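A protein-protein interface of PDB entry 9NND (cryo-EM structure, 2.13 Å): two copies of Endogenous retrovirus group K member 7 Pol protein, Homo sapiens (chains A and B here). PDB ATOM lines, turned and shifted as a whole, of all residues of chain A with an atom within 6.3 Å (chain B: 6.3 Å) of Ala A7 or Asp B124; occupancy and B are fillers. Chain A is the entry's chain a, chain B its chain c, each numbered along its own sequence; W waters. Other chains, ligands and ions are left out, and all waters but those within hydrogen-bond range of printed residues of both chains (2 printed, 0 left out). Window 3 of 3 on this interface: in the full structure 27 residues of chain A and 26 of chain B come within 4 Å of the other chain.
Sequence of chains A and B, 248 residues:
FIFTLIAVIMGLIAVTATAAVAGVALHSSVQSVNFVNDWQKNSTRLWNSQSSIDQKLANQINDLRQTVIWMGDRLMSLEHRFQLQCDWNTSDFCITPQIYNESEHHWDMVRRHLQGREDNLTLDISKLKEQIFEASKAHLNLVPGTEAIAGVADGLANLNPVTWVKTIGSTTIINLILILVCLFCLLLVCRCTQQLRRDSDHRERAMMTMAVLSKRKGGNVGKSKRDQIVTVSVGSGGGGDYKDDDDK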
ATOM      1  N   THR A   4      -3.696 -30.116  -0.729  1.00  0.00           N
ATOM      2  CA  THR A   4      -3.947 -29.137   0.322  1.00  0.00           C
ATOM      3  C   THR A   4      -5.458 -28.948   0.387  1.00  0.00           C
ATOM      4  O   THR A   4      -6.042 -28.252  -0.448  1.00  0.00           O
ATOM      5  CB  THR A   4      -3.226 -27.821   0.043  1.00  0.00           C
ATOM      6  OG1 THR A   4      -1.813 -28.050  -0.021  1.00  0.00           O
ATOM      7  CG2 THR A   4      -3.522 -26.810   1.140  1.00  0.00           C
ATOM      8  N   LEU A   5      -6.087 -29.581   1.375  1.00  0.00           N
ATOM      9  CA  LEU A   5      -7.546 -29.565   1.499  1.00  0.00           C
ATOM     10  C   LEU A   5      -7.981 -28.309   2.253  1.00  0.00           C
ATOM     11  O   LEU A   5      -8.472 -28.350   3.382  1.00  0.00           O
ATOM     12  CB  LEU A   5      -8.031 -30.836   2.185  1.00  0.00           C
ATOM     13  CG  LEU A   5      -7.516 -32.161   1.618  1.00  0.00           C
ATOM     14  CD1 LEU A   5      -7.619 -33.267   2.657  1.00  0.00           C
ATOM     15  CD2 LEU A   5      -8.273 -32.536   0.354  1.00  0.00           C
ATOM     16  N   ILE A   6      -7.792 -27.170   1.595  1.00  0.00           N
ATOM     17  CA  ILE A   6      -8.116 -25.880   2.196  1.00  0.00           C
ATOM     18  C   ILE A   6      -9.556 -25.476   1.909  1.00  0.00           C
ATOM     19  O   ILE A   6     -10.270 -25.025   2.807  1.00  0.00           O
ATOM     20  CB  ILE A   6      -7.122 -24.808   1.706  1.00  0.00           C
ATOM     21  N   ALA A   7     -10.004 -25.633   0.663  1.00  0.00           N
ATOM     22  CA  ALA A   7     -11.341 -25.198   0.281  1.00  0.00           C
ATOM     23  C   ALA A   7     -12.439 -26.121   0.791  1.00  0.00           C
ATOM     24  O   ALA A   7     -13.596 -25.694   0.869  1.00  0.00           O
ATOM     25  CB  ALA A   7     -11.437 -25.077  -1.241  1.00  0.00           C
ATOM     26  N   VAL A   8     -12.111 -27.362   1.148  1.00  0.00           N
ATOM     27  CA  VAL A   8     -13.113 -28.322   1.598  1.00  0.00           C
ATOM     28  C   VAL A   8     -13.701 -27.870   2.929  1.00  0.00           C
ATOM     29  O   VAL A   8     -13.152 -26.985   3.594  1.00  0.00           O
ATOM     30  CB  VAL A   8     -12.527 -29.742   1.712  1.00  0.00           C
ATOM     31  CG1 VAL A   8     -12.016 -30.215   0.363  1.00  0.00           C
ATOM     32  CG2 VAL A   8     -11.425 -29.783   2.755  1.00  0.00           C
ATOM     33  N   ILE A   9     -14.830 -28.465   3.318  1.00  0.00           N
ATOM     34  CA  ILE A   9     -15.502 -28.107   4.560  1.00  0.00           C
ATOM     35  C   ILE A   9     -15.161 -29.048   5.703  1.00  0.00           C
ATOM     36  O   ILE A   9     -15.634 -28.837   6.827  1.00  0.00           O
ATOM     37  CB  ILE A   9     -17.031 -28.059   4.372  1.00  0.00           C
ATOM     38  CG1 ILE A   9     -17.570 -29.453   4.052  1.00  0.00           C
ATOM     39  CG2 ILE A   9     -17.407 -27.064   3.288  1.00  0.00           C
ATOM     40  CD1 ILE A   9     -19.031 -29.627   4.385  1.00  0.00           C
ATOM     41  N   SER A  51      -9.294 -30.732  -5.616  1.00  0.00           N
ATOM     42  CA  SER A  51      -9.273 -30.047  -6.904  1.00  0.00           C
ATOM     43  C   SER A  51      -8.131 -30.523  -7.796  1.00  0.00           C
ATOM     44  O   SER A  51      -8.367 -30.960  -8.926  1.00  0.00           O
ATOM     45  CB  SER A  51      -9.182 -28.532  -6.688  1.00  0.00           C
ATOM     46  OG  SER A  51      -9.307 -27.838  -7.917  1.00  0.00           O
ATOM     47  N   HIS B 105     -22.566 -18.532  -8.626  1.00  0.00           N
ATOM     48  CA  HIS B 105     -21.402 -18.587  -9.505  1.00  0.00           C
ATOM     49  C   HIS B 105     -21.664 -17.686 -10.707  1.00  0.00           C
ATOM     50  O   HIS B 105     -22.179 -18.139 -11.730  1.00  0.00           O
ATOM     51  CB  HIS B 105     -21.113 -20.021  -9.943  1.00  0.00           C
ATOM     52  CG  HIS B 105     -20.855 -20.962  -8.809  1.00  0.00           C
ATOM     53  ND1 HIS B 105     -21.724 -21.977  -8.474  1.00  0.00           N
ATOM     54  CD2 HIS B 105     -19.822 -21.049  -7.938  1.00  0.00           C
ATOM     55  CE1 HIS B 105     -21.240 -22.645  -7.442  1.00  0.00           C
ATOM     56  NE2 HIS B 105     -20.086 -22.103  -7.099  1.00  0.00           N
ATOM     57  N   MET B 109     -16.376 -16.090 -12.750  1.00  0.00           N
ATOM     58  CA  MET B 109     -15.677 -17.209 -12.124  1.00  0.00           C
ATOM     59  C   MET B 109     -15.500 -18.362 -13.105  1.00  0.00           C
ATOM     60  O   MET B 109     -14.424 -18.966 -13.179  1.00  0.00           O
ATOM     61  CB  MET B 109     -16.435 -17.676 -10.882  1.00  0.00           C
ATOM     62  CG  MET B 109     -16.778 -16.568  -9.905  1.00  0.00           C
ATOM     63  SD  MET B 109     -17.733 -17.165  -8.500  1.00  0.00           S
ATOM     64  CE  MET B 109     -16.465 -17.205  -7.236  1.00  0.00           C
ATOM     65  N   THR B 122     -11.773 -16.939  -9.031  1.00  0.00           N
ATOM     66  CA  THR B 122     -12.055 -18.108  -9.850  1.00  0.00           C
ATOM     67  C   THR B 122     -13.079 -19.006  -9.166  1.00  0.00           C
ATOM     68  O   THR B 122     -13.208 -19.017  -7.939  1.00  0.00           O
ATOM     69  CB  THR B 122     -10.775 -18.900 -10.127  1.00  0.00           C
ATOM     70  OG1 THR B 122      -9.715 -17.998 -10.461  1.00  0.00           O
ATOM     71  CG2 THR B 122     -10.975 -19.860 -11.287  1.00  0.00           C
ATOM     72  N   LEU B 123     -13.814 -19.754  -9.985  1.00  0.00           N
ATOM     73  CA  LEU B 123     -14.742 -20.757  -9.481  1.00  0.00           C
ATOM     74  C   LEU B 123     -14.022 -21.743  -8.569  1.00  0.00           C
ATOM     75  O   LEU B 123     -12.962 -22.270  -8.913  1.00  0.00           O
ATOM     76  CB  LEU B 123     -15.388 -21.485 -10.661  1.00  0.00           C
ATOM     77  CG  LEU B 123     -16.074 -22.831 -10.436  1.00  0.00           C
ATOM     78  CD1 LEU B 123     -17.443 -22.635  -9.808  1.00  0.00           C
ATOM     79  CD2 LEU B 123     -16.190 -23.577 -11.754  1.00  0.00           C
ATOM     80  N   ASP B 124     -14.606 -21.985  -7.398  1.00  0.00           N
ATOM     81  CA  ASP B 124     -14.015 -22.864  -6.391  1.00  0.00           C
ATOM     82  C   ASP B 124     -14.363 -24.304  -6.751  1.00  0.00           C
ATOM     83  O   ASP B 124     -15.484 -24.762  -6.524  1.00  0.00           O
ATOM     84  CB  ASP B 124     -14.519 -22.494  -5.000  1.00  0.00           C
ATOM     85  CG  ASP B 124     -13.705 -23.135  -3.885  1.00  0.00           C
ATOM     86  OD1 ASP B 124     -13.138 -24.227  -4.095  1.00  0.00           O
ATOM     87  OD2 ASP B 124     -13.638 -22.543  -2.789  1.00  0.00           O
ATOM     88  N   ILE B 125     -13.387 -25.027  -7.303  1.00  0.00           N
ATOM     89  CA  ILE B 125     -13.650 -26.369  -7.813  1.00  0.00           C
ATOM     90  C   ILE B 125     -13.989 -27.330  -6.676  1.00  0.00           C
ATOM     91  O   ILE B 125     -14.865 -28.188  -6.820  1.00  0.00           O
ATOM     92  CB  ILE B 125     -12.451 -26.863  -8.645  1.00  0.00           C
ATOM     93  CG1 ILE B 125     -12.271 -25.983  -9.883  1.00  0.00           C
ATOM     94  CG2 ILE B 125     -12.641 -28.311  -9.063  1.00  0.00           C
ATOM     95  CD1 ILE B 125     -13.463 -25.987 -10.811  1.00  0.00           C
ATOM     96  N   SER B 126     -13.303 -27.212  -5.536  1.00  0.00           N
ATOM     97  CA  SER B 126     -13.558 -28.121  -4.419  1.00  0.00           C
ATOM     98  C   SER B 126     -14.974 -27.950  -3.878  1.00  0.00           C
ATOM     99  O   SER B 126     -15.684 -28.935  -3.636  1.00  0.00           O
ATOM    100  CB  SER B 126     -12.529 -27.895  -3.311  1.00  0.00           C
ATOM    101  OG  SER B 126     -11.317 -28.572  -3.590  1.00  0.00           O
ATOM    102  N   LYS B 127     -15.404 -26.703  -3.685  1.00  0.00           N
ATOM    103  CA  LYS B 127     -16.754 -26.451  -3.187  1.00  0.00           C
ATOM    104  C   LYS B 127     -17.807 -26.918  -4.186  1.00  0.00           C
ATOM    105  O   LYS B 127     -18.832 -27.497  -3.798  1.00  0.00           O
ATOM    106  CB  LYS B 127     -16.919 -24.963  -2.869  1.00  0.00           C
ATOM    107  CG  LYS B 127     -18.276 -24.591  -2.295  1.00  0.00           C
ATOM    108  CD  LYS B 127     -18.302 -23.147  -1.811  1.00  0.00           C
ATOM    109  CE  LYS B 127     -18.288 -22.164  -2.970  1.00  0.00           C
ATOM    110  NZ  LYS B 127     -19.551 -22.205  -3.757  1.00  0.00           N
ATOM    111  N   LEU B 128     -17.569 -26.675  -5.477  1.00  0.00           N
ATOM    112  CA  LEU B 128     -18.500 -27.142  -6.499  1.00  0.00           C
ATOM    113  C   LEU B 128     -18.590 -28.662  -6.506  1.00  0.00           C
ATOM    114  O   LEU B 128     -19.681 -29.224  -6.638  1.00  0.00           O
ATOM    115  CB  LEU B 128     -18.079 -26.623  -7.874  1.00  0.00           C
ATOM    116  CG  LEU B 128     -18.952 -27.075  -9.046  1.00  0.00           C
ATOM    117  CD1 LEU B 128     -20.335 -26.447  -8.957  1.00  0.00           C
ATOM    118  CD2 LEU B 128     -18.296 -26.747 -10.378  1.00  0.00           C
ATOM    119  N   LYS B 129     -17.451 -29.343  -6.369  1.00  0.00           N
ATOM    120  CA  LYS B 129     -17.460 -30.801  -6.322  1.00  0.00           C
ATOM    121  C   LYS B 129     -18.201 -31.305  -5.092  1.00  0.00           C
ATOM    122  O   LYS B 129     -18.914 -32.309  -5.161  1.00  0.00           O
ATOM    123  CB  LYS B 129     -16.032 -31.341  -6.357  1.00  0.00           C
ATOM    124  CG  LYS B 129     -15.430 -31.379  -7.748  1.00  0.00           C
ATOM    125  CD  LYS B 129     -14.020 -31.945  -7.733  1.00  0.00           C
ATOM    126  CE  LYS B 129     -13.559 -32.291  -9.136  1.00  0.00           C
ATOM    127  NZ  LYS B 129     -12.144 -32.749  -9.169  1.00  0.00           N
ATOM    128  N   GLU B 130     -18.046 -30.621  -3.956  1.00  0.00           N
ATOM    129  CA  GLU B 130     -18.817 -30.977  -2.768  1.00  0.00           C
ATOM    130  C   GLU B 130     -20.313 -30.873  -3.033  1.00  0.00           C
ATOM    131  O   GLU B 130     -21.079 -31.793  -2.718  1.00  0.00           O
ATOM    132  CB  GLU B 130     -18.432 -30.083  -1.593  1.00  0.00           C
ATOM    133  CG  GLU B 130     -17.073 -30.359  -1.019  1.00  0.00           C
ATOM    134  CD  GLU B 130     -16.754 -29.453   0.149  1.00  0.00           C
ATOM    135  OE1 GLU B 130     -17.510 -28.488   0.384  1.00  0.00           O
ATOM    136  OE2 GLU B 130     -15.761 -29.724   0.850  1.00  0.00           O
HETATM  137  O   HOH W   1     -10.195 -24.668  -7.666  1.00  0.00           O
HETATM  138  O   HOH W   2      -9.137 -28.472  -1.507  1.00  0.00           O
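The backbone NH of Ile A9 is in hydrogen-bond range of the side-chain carboxylate of Glu B130 (2.9 Å).
OD1 of Asp B124 lies within hydrogen-bond range of N of Ser B126 (3.3 Å). N of Lys B127 is in hydrogen-bond range of OD1 of Asp B124, at 3.4 Å.
Ala A7 touches Asp B124. Ala A7 touches Ser B126. Val A8 touches Glu B130. Ile B125 touches Ser A51 (CB to OG, 3.4 Å). Ser A51 touches Ser B126.
Printed residues of chain B within 4 Å of Ala A7: Asp B124 and Ser B126. Printed residues of chain B within 4 Å of Val A8: Glu B130. Printed residues of chain A within 4 Å of Ile B125: Ser A51. The nearest residue of chain B that does not touch Ala A7 is Glu B130 (4.6 Å). The nearest printed residue of chain A that does not touch Glu B130 is Ala A7 (4.6 Å).
Of the 7 printed residues of chain A, 4 touch a printed residue of chain B. Printed residues of chain B that touch a printed residue of chain A: Asp B124, Ile B125, Ser B126 and Glu B130. Among the printed residues, 6 pairs touch across the chains.
No position is printed for both chains.
Water W2 lies within hydrogen-bond range of the side-chain hydroxyl of Ser B126 (3.0 Å) and the backbone carbonyl oxygen of Thr A4 (3.3 Å). Water W1 bridges N of Ile B125 (3.2 Å) and OG of Ser A51 (3.3 Å).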
